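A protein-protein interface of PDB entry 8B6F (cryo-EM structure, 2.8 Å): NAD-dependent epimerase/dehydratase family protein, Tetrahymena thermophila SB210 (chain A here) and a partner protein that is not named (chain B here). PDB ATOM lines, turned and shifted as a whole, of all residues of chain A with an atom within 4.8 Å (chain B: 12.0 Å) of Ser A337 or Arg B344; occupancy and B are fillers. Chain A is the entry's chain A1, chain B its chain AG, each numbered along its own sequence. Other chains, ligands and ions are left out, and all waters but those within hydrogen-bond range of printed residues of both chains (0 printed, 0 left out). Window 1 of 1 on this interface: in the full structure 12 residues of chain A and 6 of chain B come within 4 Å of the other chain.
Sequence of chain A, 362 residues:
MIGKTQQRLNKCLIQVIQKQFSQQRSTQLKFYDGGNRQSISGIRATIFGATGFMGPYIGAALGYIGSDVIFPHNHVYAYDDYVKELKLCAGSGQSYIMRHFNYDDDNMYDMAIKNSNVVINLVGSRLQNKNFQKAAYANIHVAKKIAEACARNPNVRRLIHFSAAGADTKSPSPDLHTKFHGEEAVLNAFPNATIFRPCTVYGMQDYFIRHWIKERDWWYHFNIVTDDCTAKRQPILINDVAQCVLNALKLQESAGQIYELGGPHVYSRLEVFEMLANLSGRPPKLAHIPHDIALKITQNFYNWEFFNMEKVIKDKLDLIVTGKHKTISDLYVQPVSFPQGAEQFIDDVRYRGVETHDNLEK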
ATOM      1  N   TYR A 202     -15.015 -11.710 -30.925  1.00  0.00           N
ATOM      2  CA  TYR A 202     -13.860 -12.571 -31.118  1.00  0.00           C
ATOM      3  C   TYR A 202     -14.143 -13.961 -30.560  1.00  0.00           C
ATOM      4  O   TYR A 202     -14.988 -14.147 -29.680  1.00  0.00           O
ATOM      5  CB  TYR A 202     -12.605 -11.981 -30.464  1.00  0.00           C
ATOM      6  CG  TYR A 202     -12.675 -11.876 -28.964  1.00  0.00           C
ATOM      7  CD1 TYR A 202     -13.234 -10.763 -28.356  1.00  0.00           C
ATOM      8  CD2 TYR A 202     -12.169 -12.882 -28.155  1.00  0.00           C
ATOM      9  CE1 TYR A 202     -13.296 -10.657 -26.987  1.00  0.00           C
ATOM     10  CE2 TYR A 202     -12.228 -12.787 -26.781  1.00  0.00           C
ATOM     11  CZ  TYR A 202     -12.793 -11.670 -26.206  1.00  0.00           C
ATOM     12  OH  TYR A 202     -12.859 -11.558 -24.840  1.00  0.00           O
ATOM     13  N   PRO A 264     -15.713  -4.822 -21.399  1.00  0.00           N
ATOM     14  CA  PRO A 264     -15.628  -3.839 -20.307  1.00  0.00           C
ATOM     15  C   PRO A 264     -14.784  -2.621 -20.638  1.00  0.00           C
ATOM     16  O   PRO A 264     -15.076  -1.530 -20.134  1.00  0.00           O
ATOM     17  CB  PRO A 264     -15.024  -4.654 -19.154  1.00  0.00           C
ATOM     18  CG  PRO A 264     -14.316  -5.784 -19.808  1.00  0.00           C
ATOM     19  CD  PRO A 264     -15.111  -6.114 -21.031  1.00  0.00           C
ATOM     20  N   HIS A 265     -13.751  -2.764 -21.467  1.00  0.00           N
ATOM     21  CA  HIS A 265     -12.808  -1.686 -21.726  1.00  0.00           C
ATOM     22  C   HIS A 265     -12.651  -1.471 -23.224  1.00  0.00           C
ATOM     23  O   HIS A 265     -12.892  -2.369 -24.033  1.00  0.00           O
ATOM     24  CB  HIS A 265     -11.441  -1.976 -21.092  1.00  0.00           C
ATOM     25  CG  HIS A 265     -11.489  -2.120 -19.603  1.00  0.00           C
ATOM     26  ND1 HIS A 265     -11.838  -3.299 -18.980  1.00  0.00           N
ATOM     27  CD2 HIS A 265     -11.244  -1.231 -18.613  1.00  0.00           C
ATOM     28  CE1 HIS A 265     -11.800  -3.132 -17.670  1.00  0.00           C
ATOM     29  NE2 HIS A 265     -11.443  -1.886 -17.421  1.00  0.00           N
ATOM     30  N   TYR A 267     -10.138  -0.378 -26.352  1.00  0.00           N
ATOM     31  CA  TYR A 267      -8.750  -0.348 -26.783  1.00  0.00           C
ATOM     32  C   TYR A 267      -8.677   0.161 -28.213  1.00  0.00           C
ATOM     33  O   TYR A 267      -9.595  -0.047 -29.009  1.00  0.00           O
ATOM     34  CB  TYR A 267      -8.089  -1.732 -26.720  1.00  0.00           C
ATOM     35  CG  TYR A 267      -8.491  -2.576 -25.536  1.00  0.00           C
ATOM     36  CD1 TYR A 267      -9.583  -3.427 -25.606  1.00  0.00           C
ATOM     37  CD2 TYR A 267      -7.759  -2.544 -24.358  1.00  0.00           C
ATOM     38  CE1 TYR A 267      -9.947  -4.209 -24.532  1.00  0.00           C
ATOM     39  CE2 TYR A 267      -8.113  -3.324 -23.278  1.00  0.00           C
ATOM     40  CZ  TYR A 267      -9.208  -4.154 -23.372  1.00  0.00           C
ATOM     41  OH  TYR A 267      -9.569  -4.934 -22.300  1.00  0.00           O
ATOM     42  N   PRO A 335     -19.593  -8.928 -19.298  1.00  0.00           N
ATOM     43  CA  PRO A 335     -18.612  -9.468 -20.245  1.00  0.00           C
ATOM     44  C   PRO A 335     -17.235  -9.598 -19.617  1.00  0.00           C
ATOM     45  O   PRO A 335     -16.858  -8.839 -18.720  1.00  0.00           O
ATOM     46  CB  PRO A 335     -18.610  -8.439 -21.380  1.00  0.00           C
ATOM     47  CG  PRO A 335     -19.034  -7.176 -20.732  1.00  0.00           C
ATOM     48  CD  PRO A 335     -20.011  -7.563 -19.660  1.00  0.00           C
ATOM     49  N   VAL A 336     -16.480 -10.572 -20.104  1.00  0.00           N
ATOM     50  CA  VAL A 336     -15.130 -10.807 -19.605  1.00  0.00           C
ATOM     51  C   VAL A 336     -14.160  -9.893 -20.340  1.00  0.00           C
ATOM     52  O   VAL A 336     -14.371  -9.523 -21.500  1.00  0.00           O
ATOM     53  CB  VAL A 336     -14.741 -12.290 -19.758  1.00  0.00           C
ATOM     54  CG1 VAL A 336     -14.595 -12.666 -21.226  1.00  0.00           C
ATOM     55  CG2 VAL A 336     -13.460 -12.590 -18.990  1.00  0.00           C
ATOM     56  N   SER A 337     -13.080  -9.532 -19.657  1.00  0.00           N
ATOM     57  CA  SER A 337     -12.078  -8.656 -20.244  1.00  0.00           C
ATOM     58  C   SER A 337     -11.408  -9.326 -21.436  1.00  0.00           C
ATOM     59  O   SER A 337     -11.257 -10.549 -21.487  1.00  0.00           O
ATOM     60  CB  SER A 337     -11.023  -8.312 -19.203  1.00  0.00           C
ATOM     61  OG  SER A 337     -10.411  -9.510 -18.762  1.00  0.00           O
ATOM     62  N   PHE A 338     -10.993  -8.508 -22.400  1.00  0.00           N
ATOM     63  CA  PHE A 338     -10.366  -9.052 -23.602  1.00  0.00           C
ATOM     64  C   PHE A 338      -9.093  -9.828 -23.292  1.00  0.00           C
ATOM     65  O   PHE A 338      -8.927 -10.936 -23.832  1.00  0.00           O
ATOM     66  CB  PHE A 338     -10.106  -7.915 -24.595  1.00  0.00           C
ATOM     67  CG  PHE A 338      -9.372  -8.343 -25.829  1.00  0.00           C
ATOM     68  CD1 PHE A 338     -10.034  -9.010 -26.843  1.00  0.00           C
ATOM     69  CD2 PHE A 338      -8.029  -8.060 -25.987  1.00  0.00           C
ATOM     70  CE1 PHE A 338      -9.368  -9.400 -27.983  1.00  0.00           C
ATOM     71  CE2 PHE A 338      -7.355  -8.448 -27.126  1.00  0.00           C
ATOM     72  CZ  PHE A 338      -8.027  -9.117 -28.127  1.00  0.00           C
ATOM     73  N   PRO A 339      -8.169  -9.335 -22.459  1.00  0.00           N
ATOM     74  CA  PRO A 339      -6.960 -10.132 -22.179  1.00  0.00           C
ATOM     75  C   PRO A 339      -7.260 -11.509 -21.615  1.00  0.00           C
ATOM     76  O   PRO A 339      -6.574 -12.479 -21.959  1.00  0.00           O
ATOM     77  CB  PRO A 339      -6.193  -9.258 -21.177  1.00  0.00           C
ATOM     78  CG  PRO A 339      -6.698  -7.883 -21.400  1.00  0.00           C
ATOM     79  CD  PRO A 339      -8.135  -8.031 -21.777  1.00  0.00           C
ATOM     80  N   GLN A 340      -8.266 -11.622 -20.746  1.00  0.00           N
ATOM     81  CA  GLN A 340      -8.616 -12.924 -20.188  1.00  0.00           C
ATOM     82  C   GLN A 340      -9.332 -13.792 -21.213  1.00  0.00           C
ATOM     83  O   GLN A 340      -9.054 -14.990 -21.325  1.00  0.00           O
ATOM     84  CB  GLN A 340      -9.489 -12.739 -18.948  1.00  0.00           C
ATOM     85  CG  GLN A 340      -9.727 -14.015 -18.158  1.00  0.00           C
ATOM     86  CD  GLN A 340      -8.521 -14.437 -17.353  1.00  0.00           C
ATOM     87  OE1 GLN A 340      -7.499 -13.755 -17.340  1.00  0.00           O
ATOM     88  NE2 GLN A 340      -8.636 -15.567 -16.668  1.00  0.00           N
ATOM     89  N   GLY A 341     -10.257 -13.202 -21.969  1.00  0.00           N
ATOM     90  CA  GLY A 341     -11.052 -13.988 -22.897  1.00  0.00           C
ATOM     91  C   GLY A 341     -10.256 -14.537 -24.064  1.00  0.00           C
ATOM     92  O   GLY A 341     -10.456 -15.683 -24.475  1.00  0.00           O
ATOM     93  N   PRO B 336     -18.280 -13.083  -8.123  1.00  0.00           N
ATOM     94  CA  PRO B 336     -16.915 -13.515  -7.806  1.00  0.00           C
ATOM     95  C   PRO B 336     -16.225 -12.549  -6.856  1.00  0.00           C
ATOM     96  O   PRO B 336     -16.394 -11.332  -6.943  1.00  0.00           O
ATOM     97  CB  PRO B 336     -16.226 -13.551  -9.175  1.00  0.00           C
ATOM     98  CG  PRO B 336     -17.014 -12.623 -10.021  1.00  0.00           C
ATOM     99  CD  PRO B 336     -18.428 -12.736  -9.546  1.00  0.00           C
ATOM    100  N   THR B 337     -15.441 -13.111  -5.936  1.00  0.00           N
ATOM    101  CA  THR B 337     -14.643 -12.280  -5.042  1.00  0.00           C
ATOM    102  C   THR B 337     -13.443 -11.694  -5.773  1.00  0.00           C
ATOM    103  O   THR B 337     -13.073 -10.536  -5.544  1.00  0.00           O
ATOM    104  CB  THR B 337     -14.190 -13.090  -3.828  1.00  0.00           C
ATOM    105  OG1 THR B 337     -13.365 -14.183  -4.257  1.00  0.00           O
ATOM    106  CG2 THR B 337     -15.391 -13.632  -3.066  1.00  0.00           C
ATOM    107  N   ASN B 338     -12.825 -12.476  -6.653  1.00  0.00           N
ATOM    108  CA  ASN B 338     -11.716 -12.008  -7.482  1.00  0.00           C
ATOM    109  C   ASN B 338     -12.297 -11.547  -8.811  1.00  0.00           C
ATOM    110  O   ASN B 338     -12.565 -12.358  -9.701  1.00  0.00           O
ATOM    111  CB  ASN B 338     -10.683 -13.111  -7.673  1.00  0.00           C
ATOM    112  CG  ASN B 338      -9.560 -12.703  -8.604  1.00  0.00           C
ATOM    113  OD1 ASN B 338      -9.331 -11.517  -8.835  1.00  0.00           O
ATOM    114  ND2 ASN B 338      -8.852 -13.687  -9.143  1.00  0.00           N
ATOM    115  N   LYS B 339     -12.485 -10.238  -8.951  1.00  0.00           N
ATOM    116  CA  LYS B 339     -13.117  -9.656 -10.125  1.00  0.00           C
ATOM    117  C   LYS B 339     -12.112  -9.256 -11.195  1.00  0.00           C
ATOM    118  O   LYS B 339     -12.500  -8.635 -12.189  1.00  0.00           O
ATOM    119  CB  LYS B 339     -13.956  -8.442  -9.719  1.00  0.00           C
ATOM    120  CG  LYS B 339     -15.032  -8.758  -8.692  1.00  0.00           C
ATOM    121  CD  LYS B 339     -15.779  -7.507  -8.259  1.00  0.00           C
ATOM    122  CE  LYS B 339     -16.823  -7.831  -7.201  1.00  0.00           C
ATOM    123  NZ  LYS B 339     -17.561  -6.616  -6.755  1.00  0.00           N
ATOM    124  N   LYS B 340     -10.838  -9.593 -11.017  1.00  0.00           N
ATOM    125  CA  LYS B 340      -9.833  -9.250 -12.016  1.00  0.00           C
ATOM    126  C   LYS B 340     -10.194  -9.727 -13.415  1.00  0.00           C
ATOM    127  O   LYS B 340     -10.024  -8.943 -14.363  1.00  0.00           O
ATOM    128  CB  LYS B 340      -8.469  -9.819 -11.600  1.00  0.00           C
ATOM    129  CG  LYS B 340      -7.858  -9.141 -10.388  1.00  0.00           C
ATOM    130  CD  LYS B 340      -6.469  -9.687 -10.102  1.00  0.00           C
ATOM    131  CE  LYS B 340      -5.809  -8.940  -8.956  1.00  0.00           C
ATOM    132  NZ  LYS B 340      -4.429  -9.438  -8.693  1.00  0.00           N
ATOM    133  N   PRO B 341     -10.678 -10.953 -13.624  1.00  0.00           N
ATOM    134  CA  PRO B 341     -10.977 -11.379 -15.001  1.00  0.00           C
ATOM    135  C   PRO B 341     -11.946 -10.461 -15.719  1.00  0.00           C
ATOM    136  O   PRO B 341     -11.800 -10.238 -16.927  1.00  0.00           O
ATOM    137  CB  PRO B 341     -11.561 -12.786 -14.807  1.00  0.00           C
ATOM    138  CG  PRO B 341     -11.011 -13.252 -13.513  1.00  0.00           C
ATOM    139  CD  PRO B 341     -10.912 -12.033 -12.651  1.00  0.00           C
ATOM    140  N   TRP B 342     -12.939  -9.924 -15.013  1.00  0.00           N
ATOM    141  CA  TRP B 342     -13.949  -9.068 -15.618  1.00  0.00           C
ATOM    142  C   TRP B 342     -13.688  -7.584 -15.401  1.00  0.00           C
ATOM    143  O   TRP B 342     -14.487  -6.762 -15.855  1.00  0.00           O
ATOM    144  CB  TRP B 342     -15.334  -9.429 -15.068  1.00  0.00           C
ATOM    145  CG  TRP B 342     -15.672 -10.877 -15.227  1.00  0.00           C
ATOM    146  CD1 TRP B 342     -16.320 -11.456 -16.278  1.00  0.00           C
ATOM    147  CD2 TRP B 342     -15.374 -11.933 -14.308  1.00  0.00           C
ATOM    148  NE1 TRP B 342     -16.445 -12.807 -16.069  1.00  0.00           N
ATOM    149  CE2 TRP B 342     -15.873 -13.125 -14.866  1.00  0.00           C
ATOM    150  CE3 TRP B 342     -14.735 -11.986 -13.065  1.00  0.00           C
ATOM    151  CZ2 TRP B 342     -15.752 -14.355 -14.227  1.00  0.00           C
ATOM    152  CZ3 TRP B 342     -14.616 -13.208 -12.432  1.00  0.00           C
ATOM    153  CH2 TRP B 342     -15.123 -14.377 -13.013  1.00  0.00           C
ATOM    154  N   THR B 343     -12.597  -7.218 -14.719  1.00  0.00           N
ATOM    155  CA  THR B 343     -12.304  -5.816 -14.438  1.00  0.00           C
ATOM    156  C   THR B 343     -10.857  -5.447 -14.754  1.00  0.00           C
ATOM    157  O   THR B 343     -10.381  -4.402 -14.299  1.00  0.00           O
ATOM    158  CB  THR B 343     -12.613  -5.483 -12.976  1.00  0.00           C
ATOM    159  OG1 THR B 343     -11.810  -6.299 -12.114  1.00  0.00           O
ATOM    160  CG2 THR B 343     -14.083  -5.724 -12.670  1.00  0.00           C
ATOM    161  N   ARG B 344     -10.149  -6.272 -15.518  1.00  0.00           N
ATOM    162  CA  ARG B 344      -8.786  -5.981 -15.938  1.00  0.00           C
ATOM    163  C   ARG B 344      -8.796  -5.463 -17.369  1.00  0.00           C
ATOM    164  O   ARG B 344      -9.510  -5.991 -18.224  1.00  0.00           O
ATOM    165  CB  ARG B 344      -7.891  -7.217 -15.832  1.00  0.00           C
ATOM    166  CG  ARG B 344      -8.302  -8.338 -16.753  1.00  0.00           C
ATOM    167  CD  ARG B 344      -7.394  -9.551 -16.661  1.00  0.00           C
ATOM    168  NE  ARG B 344      -6.072  -9.281 -17.213  1.00  0.00           N
ATOM    169  CZ  ARG B 344      -5.156 -10.208 -17.452  1.00  0.00           C
ATOM    170  NH1 ARG B 344      -5.384 -11.487 -17.201  1.00  0.00           N
ATOM    171  NH2 ARG B 344      -3.984  -9.844 -17.962  1.00  0.00           N
ATOM    172  N   LYS B 345      -8.006  -4.424 -17.624  1.00  0.00           N
ATOM    173  CA  LYS B 345      -7.871  -3.872 -18.966  1.00  0.00           C
ATOM    174  C   LYS B 345      -6.662  -4.418 -19.709  1.00  0.00           C
ATOM    175  O   LYS B 345      -6.768  -4.741 -20.896  1.00  0.00           O
ATOM    176  CB  LYS B 345      -7.779  -2.343 -18.905  1.00  0.00           C
ATOM    177  CG  LYS B 345      -7.837  -1.673 -20.269  1.00  0.00           C
ATOM    178  CD  LYS B 345      -7.844  -0.160 -20.147  1.00  0.00           C
ATOM    179  CE  LYS B 345      -7.862   0.501 -21.515  1.00  0.00           C
ATOM    180  NZ  LYS B 345      -7.827   1.988 -21.418  1.00  0.00           N
ATOM    181  N   TYR B 346      -5.518  -4.533 -19.043  1.00  0.00           N
ATOM    182  CA  TYR B 346      -4.314  -5.065 -19.670  1.00  0.00           C
ATOM    183  C   TYR B 346      -3.835  -6.314 -18.943  1.00  0.00           C
ATOM    184  O   TYR B 346      -3.218  -7.194 -19.537  1.00  0.00           O
ATOM    185  CB  TYR B 346      -3.207  -4.012 -19.682  1.00  0.00           C
ATOM    186  CG  TYR B 346      -3.579  -2.743 -20.408  1.00  0.00           C
ATOM    187  CD1 TYR B 346      -3.482  -2.657 -21.790  1.00  0.00           C
ATOM    188  CD2 TYR B 346      -4.025  -1.630 -19.709  1.00  0.00           C
ATOM    189  CE1 TYR B 346      -3.821  -1.497 -22.458  1.00  0.00           C
ATOM    190  CE2 TYR B 346      -4.367  -0.466 -20.367  1.00  0.00           C
ATOM    191  CZ  TYR B 346      -4.263  -0.406 -21.741  1.00  0.00           C
ATOM    192  OH  TYR B 346      -4.600   0.753 -22.400  1.00  0.00           O
ATOM    193  OXT TYR B 346      -4.056  -6.473 -17.743  1.00  0.00           O
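OG of Ser A337 is in hydrogen-bond range of O of Pro B341. The guanidinium group (NH1) of Arg B344 is in hydrogen-bond range of the side-chain amide oxygen (OE1) of Gln A340, 3.1 Å away. O of Lys B345 lies close to OH of Tyr A267 (3.1 Å).
The backbone carbonyl oxygen (O) of Lys B339 is in hydrogen-bond range of the side-chain hydroxyl (OG1) of Thr B343 (2.4 Å). The chain-end carboxylate of Tyr B346 is in salt-bridge range of the guanidinium group of Arg B344.
Among the printed residues, pairs that only touch across the chains: Pro A264 with Trp B342, His A265 with Thr B343, His A265 with Arg B344, His A265 with Lys B345, Pro A335 with Trp B342, Val A336 with Pro B341, Val A336 with Trp B342, Ser A337 with Arg B344, Pro A339 with Arg B344, Pro A339 with Lys B345, Pro A339 with Tyr B346 and Gln A340 with Pro B341.
Of chain B, only Pro B341 (2.4 Å) and Arg B344 (2.9 Å) come within 4 Å of Ser A337. Arg B344 touches four residues of chain A. Pro A264 touches one residue of chain B. His A265 touches three residues of chain B. Of chain B, only Trp B342 (3.6 Å) comes within 4 Å of Pro A335. Of chain B, only Pro B341 and Trp B342 come within 4 Å of Val A336. Of the printed residues of chain B, Pro A339 touches Arg B344, Lys B345 and Tyr B346. Printed residues of chain B within 4 Å of Gln A340: Pro B341 and Arg B344. Of the printed residues of chain A, Lys B345 touches His A265, Tyr A267 and Pro A339. Printed residues of chain A within 4 Å of Tyr B346: Pro A339. Asn B338 touches none of the printed residues of chain A. Tyr A202 touches none of the printed residues of chain B. The nearest residue of chain B that does not touch Ser A337 is Trp B342 (4.2 Å). The nearest residue of chain A that does not touch Arg B344 is Tyr A267 (4.2 Å). The nearest printed residue of chain A that does not touch Thr B343 is Ser A337 (4.9 Å).
Printed residues of chain B that touch a printed residue of chain A: Pro B341, Trp B342, Thr B343, Arg B344, Lys B345 and Tyr B346. Hydrophobic or aromatic side chains of chain B within 4 Å of the printed part of chain A: Trp B342. Of the 11 printed residues of chain A, 8 touch a printed residue of chain B. Hydrophobic or aromatic side chains of chain A within 4 Å of the printed part of chain B: Pro A264, His A265, Tyr A267, Val A336 and Pro A339. Among the printed residues, 15 pairs touch across the chains. Among the printed residues, no Asp or Glu carboxylate lies within 4 Å of a Lys or Arg side-chain nitrogen of the other chain.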
